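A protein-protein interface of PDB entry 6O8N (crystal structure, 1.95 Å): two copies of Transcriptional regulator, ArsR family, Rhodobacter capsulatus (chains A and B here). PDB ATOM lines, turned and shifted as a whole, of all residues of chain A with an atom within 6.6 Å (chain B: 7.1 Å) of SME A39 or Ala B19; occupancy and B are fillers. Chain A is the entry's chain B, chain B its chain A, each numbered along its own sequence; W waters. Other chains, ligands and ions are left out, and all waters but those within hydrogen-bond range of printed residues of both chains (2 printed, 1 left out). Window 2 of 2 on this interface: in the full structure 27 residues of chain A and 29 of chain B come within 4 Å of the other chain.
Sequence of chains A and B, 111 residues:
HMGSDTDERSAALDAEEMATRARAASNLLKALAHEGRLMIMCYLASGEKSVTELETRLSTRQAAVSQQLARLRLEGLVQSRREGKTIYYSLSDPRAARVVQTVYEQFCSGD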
ATOM      1  N   LEU A  32      -9.611  36.732  24.812  1.00  0.00           N
ATOM      2  CA  LEU A  32      -8.475  35.856  24.552  1.00  0.00           C
ATOM      3  C   LEU A  32      -7.975  35.148  25.802  1.00  0.00           C
ATOM      4  O   LEU A  32      -7.354  34.087  25.687  1.00  0.00           O
ATOM      5  CB  LEU A  32      -7.328  36.653  23.927  1.00  0.00           C
ATOM      6  CG  LEU A  32      -7.592  37.271  22.553  1.00  0.00           C
ATOM      7  CD1 LEU A  32      -6.400  38.095  22.099  1.00  0.00           C
ATOM      8  CD2 LEU A  32      -7.926  36.198  21.526  1.00  0.00           C
ATOM      9  N   HIS A  34      -8.726  33.040  27.998  1.00  0.00           N
ATOM     10  CA  HIS A  34      -9.293  31.779  28.455  1.00  0.00           C
ATOM     11  C   HIS A  34      -8.439  30.646  27.917  1.00  0.00           C
ATOM     12  O   HIS A  34      -8.117  30.623  26.724  1.00  0.00           O
ATOM     13  CB  HIS A  34     -10.744  31.621  27.993  1.00  0.00           C
ATOM     14  CG  HIS A  34     -11.648  32.719  28.461  1.00  0.00           C
ATOM     15  ND1 HIS A  34     -12.241  32.713  29.704  1.00  0.00           N
ATOM     16  CD2 HIS A  34     -12.056  33.858  27.852  1.00  0.00           C
ATOM     17  CE1 HIS A  34     -12.979  33.800  29.841  1.00  0.00           C
ATOM     18  NE2 HIS A  34     -12.884  34.512  28.732  1.00  0.00           N
ATOM     19  N   GLU A  35      -8.068  29.714  28.798  1.00  0.00           N
ATOM     20  CA  GLU A  35      -6.921  28.852  28.534  1.00  0.00           C
ATOM     21  C   GLU A  35      -7.179  27.952  27.332  1.00  0.00           C
ATOM     22  O   GLU A  35      -6.356  27.872  26.413  1.00  0.00           O
ATOM     23  CB  GLU A  35      -6.592  28.019  29.773  1.00  0.00           C
ATOM     24  CG  GLU A  35      -5.320  28.449  30.483  1.00  0.00           C
ATOM     25  CD  GLU A  35      -5.122  27.744  31.810  1.00  0.00           C
ATOM     26  OE1 GLU A  35      -4.617  28.387  32.755  1.00  0.00           O
ATOM     27  OE2 GLU A  35      -5.470  26.548  31.907  1.00  0.00           O
ATOM     28  N   GLY A  36      -8.328  27.274  27.314  1.00  0.00           N
ATOM     29  CA  GLY A  36      -8.617  26.363  26.219  1.00  0.00           C
ATOM     30  C   GLY A  36      -8.806  27.075  24.894  1.00  0.00           C
ATOM     31  O   GLY A  36      -8.337  26.605  23.853  1.00  0.00           O
ATOM     32  N   ARG A  37      -9.498  28.218  24.910  1.00  0.00           N
ATOM     33  CA  ARG A  37      -9.718  28.963  23.674  1.00  0.00           C
ATOM     34  C   ARG A  37      -8.414  29.531  23.130  1.00  0.00           C
ATOM     35  O   ARG A  37      -8.190  29.534  21.913  1.00  0.00           O
ATOM     36  CB  ARG A  37     -10.732  30.083  23.907  1.00  0.00           C
ATOM     37  CG  ARG A  37     -12.172  29.685  23.632  1.00  0.00           C
ATOM     38  CD  ARG A  37     -13.141  30.677  24.250  1.00  0.00           C
ATOM     39  NE  ARG A  37     -13.328  30.440  25.679  1.00  0.00           N
ATOM     40  CZ  ARG A  37     -14.087  31.194  26.467  1.00  0.00           C
ATOM     41  NH1 ARG A  37     -14.729  32.242  25.967  1.00  0.00           N
ATOM     42  NH2 ARG A  37     -14.203  30.903  27.756  1.00  0.00           N
ATOM     43  N   LEU A  38      -7.543  30.013  24.009  1.00  0.00           N
ATOM     44  CA  LEU A  38      -6.263  30.565  23.586  1.00  0.00           C
ATOM     45  C   LEU A  38      -5.359  29.474  23.021  1.00  0.00           C
ATOM     46  O   LEU A  38      -4.590  29.718  22.097  1.00  0.00           O
ATOM     47  CB  LEU A  38      -5.570  31.274  24.752  1.00  0.00           C
ATOM     48  CG  LEU A  38      -4.344  32.107  24.375  1.00  0.00           C
ATOM     49  CD1 LEU A  38      -4.734  33.247  23.449  1.00  0.00           C
ATOM     50  CD2 LEU A  38      -3.647  32.632  25.621  1.00  0.00           C
ATOM     51  N   SME A  39      -5.467  28.269  23.573  1.00  0.00           N
ATOM     52  CA  SME A  39      -4.724  27.132  23.071  1.00  0.00           C
ATOM     53  CB  SME A  39      -5.003  25.821  23.827  1.00  0.00           C
ATOM     54  CG  SME A  39      -4.406  25.854  25.206  1.00  0.00           C
ATOM     55  S   SME A  39      -4.665  24.308  26.010  1.00  0.00           S
ATOM     56  OE  SME A  39      -4.254  24.530  27.424  1.00  0.00           O
ATOM     57  CE  SME A  39      -3.356  23.454  25.256  1.00  0.00           C
ATOM     58  C   SME A  39      -5.028  26.882  21.601  1.00  0.00           C
ATOM     59  O   SME A  39      -4.182  26.559  20.766  1.00  0.00           O
ATOM     60  N   ILE A  40      -6.304  27.049  21.269  1.00  0.00           N
ATOM     61  CA  ILE A  40      -6.754  26.958  19.884  1.00  0.00           C
ATOM     62  C   ILE A  40      -6.188  28.105  19.052  1.00  0.00           C
ATOM     63  O   ILE A  40      -5.664  27.888  17.958  1.00  0.00           O
ATOM     64  CB  ILE A  40      -8.291  26.932  19.805  1.00  0.00           C
ATOM     65  CG1 ILE A  40      -8.835  25.679  20.494  1.00  0.00           C
ATOM     66  CG2 ILE A  40      -8.755  26.992  18.355  1.00  0.00           C
ATOM     67  CD1 ILE A  40     -10.344  25.645  20.597  1.00  0.00           C
ATOM     68  N   MET A  41      -6.295  29.324  19.573  1.00  0.00           N
ATOM     69  CA  MET A  41      -5.826  30.507  18.860  1.00  0.00           C
ATOM     70  C   MET A  41      -4.321  30.450  18.611  1.00  0.00           C
ATOM     71  O   MET A  41      -3.844  30.876  17.559  1.00  0.00           O
ATOM     72  CB  MET A  41      -6.179  31.779  19.637  1.00  0.00           C
ATOM     73  CG  MET A  41      -7.673  32.027  19.789  1.00  0.00           C
ATOM     74  SD  MET A  41      -8.498  32.365  18.222  1.00  0.00           S
ATOM     75  CE  MET A  41      -8.072  34.086  17.974  1.00  0.00           C
ATOM     76  N   CSS A  42      -3.582  29.917  19.581  1.00  0.00           N
ATOM     77  CA  CSS A  42      -2.137  29.795  19.464  1.00  0.00           C
ATOM     78  CB  CSS A  42      -1.514  29.358  20.788  1.00  0.00           C
ATOM     79  SG  CSS A  42      -1.699  30.616  22.010  1.00  0.00           S
ATOM     80  SD  CSS A  42      -0.039  31.717  21.680  1.00  0.00           S
ATOM     81  C   CSS A  42      -1.784  28.807  18.389  1.00  0.00           C
ATOM     82  O   CSS A  42      -0.805  29.020  17.645  1.00  0.00           O
ATOM     83  N   TYR A  43      -2.555  27.728  18.289  1.00  0.00           N
ATOM     84  CA  TYR A  43      -2.319  26.715  17.267  1.00  0.00           C
ATOM     85  C   TYR A  43      -2.627  27.257  15.875  1.00  0.00           C
ATOM     86  O   TYR A  43      -1.892  27.001  14.921  1.00  0.00           O
ATOM     87  CB  TYR A  43      -3.159  25.467  17.545  1.00  0.00           C
ATOM     88  CG  TYR A  43      -2.447  24.437  18.392  1.00  0.00           C
ATOM     89  CD1 TYR A  43      -1.112  24.130  18.165  1.00  0.00           C
ATOM     90  CD2 TYR A  43      -3.107  23.773  19.417  1.00  0.00           C
ATOM     91  CE1 TYR A  43      -0.454  23.192  18.937  1.00  0.00           C
ATOM     92  CE2 TYR A  43      -2.457  22.831  20.194  1.00  0.00           C
ATOM     93  CZ  TYR A  43      -1.131  22.544  19.948  1.00  0.00           C
ATOM     94  OH  TYR A  43      -0.478  21.609  20.718  1.00  0.00           O
ATOM     95  N   LEU A  44      -3.718  28.017  15.765  1.00  0.00           N
ATOM     96  CA  LEU A  44      -4.060  28.643  14.494  1.00  0.00           C
ATOM     97  C   LEU A  44      -3.081  29.746  14.110  1.00  0.00           C
ATOM     98  O   LEU A  44      -3.039  30.138  12.939  1.00  0.00           O
ATOM     99  CB  LEU A  44      -5.483  29.204  14.550  1.00  0.00           C
ATOM    100  CG  LEU A  44      -6.603  28.192  14.799  1.00  0.00           C
ATOM    101  CD1 LEU A  44      -7.968  28.837  14.611  1.00  0.00           C
ATOM    102  CD2 LEU A  44      -6.452  26.984  13.884  1.00  0.00           C
ATOM    103  N   LEU A  54      -6.464  19.660  15.583  1.00  0.00           N
ATOM    104  CA  LEU A  54      -6.754  20.374  16.824  1.00  0.00           C
ATOM    105  C   LEU A  54      -7.107  19.403  17.943  1.00  0.00           C
ATOM    106  O   LEU A  54      -6.515  19.444  19.027  1.00  0.00           O
ATOM    107  CB  LEU A  54      -7.887  21.376  16.602  1.00  0.00           C
ATOM    108  CG  LEU A  54      -7.512  22.696  15.924  1.00  0.00           C
ATOM    109  CD1 LEU A  54      -8.739  23.581  15.749  1.00  0.00           C
ATOM    110  CD2 LEU A  54      -6.432  23.420  16.715  1.00  0.00           C
ATOM    111  N   ARG A  57      -4.147  17.472  19.157  1.00  0.00           N
ATOM    112  CA  ARG A  57      -3.093  18.157  19.894  1.00  0.00           C
ATOM    113  C   ARG A  57      -3.521  18.554  21.300  1.00  0.00           C
ATOM    114  O   ARG A  57      -2.659  18.726  22.169  1.00  0.00           O
ATOM    115  CB  ARG A  57      -2.639  19.399  19.124  1.00  0.00           C
ATOM    116  CG  ARG A  57      -1.632  19.115  18.021  1.00  0.00           C
ATOM    117  CD  ARG A  57      -1.394  20.352  17.170  1.00  0.00           C
ATOM    118  NE  ARG A  57      -1.458  20.070  15.739  1.00  0.00           N
ATOM    119  CZ  ARG A  57      -0.681  20.649  14.830  1.00  0.00           C
ATOM    120  NH1 ARG A  57       0.221  21.547  15.202  1.00  0.00           N
ATOM    121  NH2 ARG A  57      -0.807  20.335  13.548  1.00  0.00           N
ATOM    122  N   LEU A  58      -4.819  18.699  21.543  1.00  0.00           N
ATOM    123  CA  LEU A  58      -5.325  19.273  22.782  1.00  0.00           C
ATOM    124  C   LEU A  58      -5.687  18.174  23.772  1.00  0.00           C
ATOM    125  O   LEU A  58      -6.155  17.097  23.392  1.00  0.00           O
ATOM    126  CB  LEU A  58      -6.548  20.155  22.514  1.00  0.00           C
ATOM    127  CG  LEU A  58      -6.296  21.414  21.686  1.00  0.00           C
ATOM    128  CD1 LEU A  58      -7.585  21.912  21.047  1.00  0.00           C
ATOM    129  CD2 LEU A  58      -5.661  22.497  22.538  1.00  0.00           C
ATOM    130  N   SER A  59      -5.467  18.459  25.056  1.00  0.00           N
ATOM    131  CA  SER A  59      -5.978  17.617  26.131  1.00  0.00           C
ATOM    132  C   SER A  59      -7.461  17.831  26.399  1.00  0.00           C
ATOM    133  O   SER A  59      -7.998  17.220  27.330  1.00  0.00           O
ATOM    134  CB  SER A  59      -5.187  17.864  27.420  1.00  0.00           C
ATOM    135  OG  SER A  59      -3.813  18.076  27.142  1.00  0.00           O
ATOM    136  N   THR A  60      -8.131  18.674  25.621  1.00  0.00           N
ATOM    137  CA  THR A  60      -9.519  19.027  25.875  1.00  0.00           C
ATOM    138  C   THR A  60     -10.449  18.056  25.159  1.00  0.00           C
ATOM    139  O   THR A  60     -10.106  17.488  24.119  1.00  0.00           O
ATOM    140  CB  THR A  60      -9.808  20.458  25.419  1.00  0.00           C
ATOM    141  OG1 THR A  60      -8.673  21.290  25.699  1.00  0.00           O
ATOM    142  CG2 THR A  60     -11.028  21.015  26.138  1.00  0.00           C
ATOM    143  N   GLU B  16       2.223  18.420  27.770  1.00  0.00           N
ATOM    144  CA  GLU B  16       2.734  18.949  26.512  1.00  0.00           C
ATOM    145  C   GLU B  16       3.339  20.336  26.726  1.00  0.00           C
ATOM    146  O   GLU B  16       2.780  21.158  27.452  1.00  0.00           O
ATOM    147  CB  GLU B  16       1.615  18.996  25.464  1.00  0.00           C
ATOM    148  CG  GLU B  16       1.897  19.893  24.274  1.00  0.00           C
ATOM    149  CD  GLU B  16       3.066  19.402  23.446  1.00  0.00           C
ATOM    150  OE1 GLU B  16       4.009  20.189  23.222  1.00  0.00           O
ATOM    151  OE2 GLU B  16       3.045  18.229  23.021  1.00  0.00           O
ATOM    152  N   GLU B  17       4.490  20.579  26.101  1.00  0.00           N
ATOM    153  CA  GLU B  17       5.186  21.862  26.209  1.00  0.00           C
ATOM    154  C   GLU B  17       4.314  23.010  25.701  1.00  0.00           C
ATOM    155  O   GLU B  17       4.276  24.091  26.294  1.00  0.00           O
ATOM    156  CB  GLU B  17       6.507  21.829  25.428  1.00  0.00           C
ATOM    157  CG  GLU B  17       7.707  21.357  26.232  1.00  0.00           C
ATOM    158  CD  GLU B  17       8.159  22.368  27.268  1.00  0.00           C
ATOM    159  OE1 GLU B  17       9.140  23.095  26.997  1.00  0.00           O
ATOM    160  OE2 GLU B  17       7.537  22.423  28.353  1.00  0.00           O
ATOM    161  N   SME B  18       3.628  22.766  24.590  1.00  0.00           N
ATOM    162  CA  SME B  18       2.886  23.796  23.899  1.00  0.00           C
ATOM    163  CB  SME B  18       2.316  23.332  22.541  1.00  0.00           C
ATOM    164  CG  SME B  18       1.310  24.284  21.949  1.00  0.00           C
ATOM    165  S   SME B  18       2.123  25.720  21.323  1.00  0.00           S
ATOM    166  OE  SME B  18       1.213  26.236  20.262  1.00  0.00           O
ATOM    167  CE  SME B  18       3.448  24.979  20.478  1.00  0.00           C
ATOM    168  C   SME B  18       1.748  24.266  24.791  1.00  0.00           C
ATOM    169  O   SME B  18       1.340  25.430  24.862  1.00  0.00           O
ATOM    170  N   ALA B  19       1.227  23.298  25.539  1.00  0.00           N
ATOM    171  CA  ALA B  19       0.121  23.536  26.459  1.00  0.00           C
ATOM    172  C   ALA B  19       0.518  24.454  27.613  1.00  0.00           C
ATOM    173  O   ALA B  19      -0.237  25.351  27.982  1.00  0.00           O
ATOM    174  CB  ALA B  19      -0.403  22.213  26.995  1.00  0.00           C
ATOM    175  N   THR B  20       1.704  24.228  28.188  1.00  0.00           N
ATOM    176  CA  THR B  20       2.146  25.066  29.298  1.00  0.00           C
ATOM    177  C   THR B  20       2.486  26.478  28.841  1.00  0.00           C
ATOM    178  O   THR B  20       2.319  27.434  29.607  1.00  0.00           O
ATOM    179  CB  THR B  20       3.356  24.443  29.995  1.00  0.00           C
ATOM    180  OG1 THR B  20       4.552  24.798  29.288  1.00  0.00           O
ATOM    181  CG2 THR B  20       3.231  22.930  30.041  1.00  0.00           C
ATOM    182  N   ARG B  21       2.967  26.630  27.605  1.00  0.00           N
ATOM    183  CA  ARG B  21       3.218  27.965  27.069  1.00  0.00           C
ATOM    184  C   ARG B  21       1.919  28.741  26.901  1.00  0.00           C
ATOM    185  O   ARG B  21       1.877  29.954  27.140  1.00  0.00           O
ATOM    186  CB  ARG B  21       3.964  27.862  25.739  1.00  0.00           C
ATOM    187  CG  ARG B  21       5.336  27.208  25.857  1.00  0.00           C
ATOM    188  CD  ARG B  21       6.002  27.023  24.500  1.00  0.00           C
ATOM    189  NE  ARG B  21       7.432  26.748  24.628  1.00  0.00           N
ATOM    190  CZ  ARG B  21       8.234  26.459  23.608  1.00  0.00           C
ATOM    191  NH1 ARG B  21       7.750  26.406  22.375  1.00  0.00           N
ATOM    192  NH2 ARG B  21       9.522  26.222  23.819  1.00  0.00           N
ATOM    193  N   ALA B  22       0.848  28.053  26.504  1.00  0.00           N
ATOM    194  CA  ALA B  22      -0.449  28.709  26.379  1.00  0.00           C
ATOM    195  C   ALA B  22      -0.950  29.208  27.728  1.00  0.00           C
ATOM    196  O   ALA B  22      -1.507  30.310  27.820  1.00  0.00           O
ATOM    197  CB  ALA B  22      -1.457  27.752  25.746  1.00  0.00           C
ATOM    198  N   ARG B  23      -0.753  28.420  28.790  1.00  0.00           N
ATOM    199  CA  ARG B  23      -1.207  28.838  30.114  1.00  0.00           C
ATOM    200  C   ARG B  23      -0.458  30.077  30.591  1.00  0.00           C
ATOM    201  O   ARG B  23      -1.043  30.958  31.232  1.00  0.00           O
ATOM    202  CB  ARG B  23      -1.039  27.691  31.110  1.00  0.00           C
ATOM    203  CG  ARG B  23      -1.706  26.398  30.666  1.00  0.00           C
ATOM    204  CD  ARG B  23      -1.936  25.451  31.832  1.00  0.00           C
ATOM    205  NE  ARG B  23      -0.683  25.028  32.449  1.00  0.00           N
ATOM    206  CZ  ARG B  23       0.049  24.000  32.031  1.00  0.00           C
ATOM    207  NH1 ARG B  23      -0.349  23.277  30.991  1.00  0.00           N
ATOM    208  NH2 ARG B  23       1.176  23.690  32.657  1.00  0.00           N
ATOM    209  N   ALA B  24       0.838  30.166  30.282  1.00  0.00           N
ATOM    210  CA  ALA B  24       1.604  31.356  30.639  1.00  0.00           C
ATOM    211  C   ALA B  24       1.178  32.561  29.809  1.00  0.00           C
ATOM    212  O   ALA B  24       1.060  33.674  30.336  1.00  0.00           O
ATOM    213  CB  ALA B  24       3.099  31.086  30.473  1.00  0.00           C
ATOM    214  N   SER B  26      -1.870  32.718  28.653  1.00  0.00           N
ATOM    215  CA  SER B  26      -3.184  32.964  29.242  1.00  0.00           C
ATOM    216  C   SER B  26      -3.080  33.813  30.503  1.00  0.00           C
ATOM    217  O   SER B  26      -3.880  34.734  30.708  1.00  0.00           O
ATOM    218  CB  SER B  26      -3.878  31.640  29.554  1.00  0.00           C
ATOM    219  OG  SER B  26      -5.121  31.862  30.202  1.00  0.00           O
HETATM  220  O   HOH W   1       0.251  27.771  23.450  1.00  0.00           O
HETATM  221  O   HOH W   2      -1.768  25.968  22.042  1.00  0.00           O
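OE1 of Glu B16 is in hydrogen-bond range of N of SME B18 (2.9 Å).
Among the printed residues, pairs that only touch across the chains: Glu A35 with Arg B23 (3.7 Å), Glu A35 with Ser B26 (3.4 Å), Leu A38 with Ala B22 (3.8 Å), Leu A38 with Ser B26 (3.5 Å), SME A39 with Ala B19 (3.6 Å), SME A39 with Ala B22 (3.5 Å) and Tyr A43 with SME B18 (3.4 Å).
Printed residues of chain B within 4 Å of SME A39: Ala B19 and Ala B22. Of chain A, only SME A39 comes within 4 Å of Ala B19. Printed residues of chain B within 4 Å of Leu A38: Ala B22 and Ser B26. Printed residues of chain B within 4 Å of Glu A35: Arg B23 (3.7 Å) and Ser B26 (3.4 Å). Of the printed residues of chain A, Arg B23 touches Glu A35 (3.7 Å). Of the printed residues of chain A, SME B18 touches Tyr A43 (3.4 Å).
Hydrophobic or aromatic side chains of chain A that line the printed part of chain B: Leu A38 and Tyr A43. Hydrophobic or aromatic side chains of chain B that line the printed part of chain A: Ala B19 and Ala B22. Among the printed residues, no Asp or Glu carboxylate lies within 4 Å of a Lys or Arg side-chain nitrogen of the other chain.
No position is printed for both chains. Of the 7 pairs that touch across the chains among the printed residues, none has its exchanged pair printed and touching as well.
Water W2 lies within hydrogen-bond range of O of SME A39 (2.8 Å) and OE of SME B18 (3.5 Å). Water W1 lies within hydrogen-bond range of O of SME B18 (2.9 Å), N of Ala B22 (3.1 Å) and SG of CSS A42 (3.7 Å).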
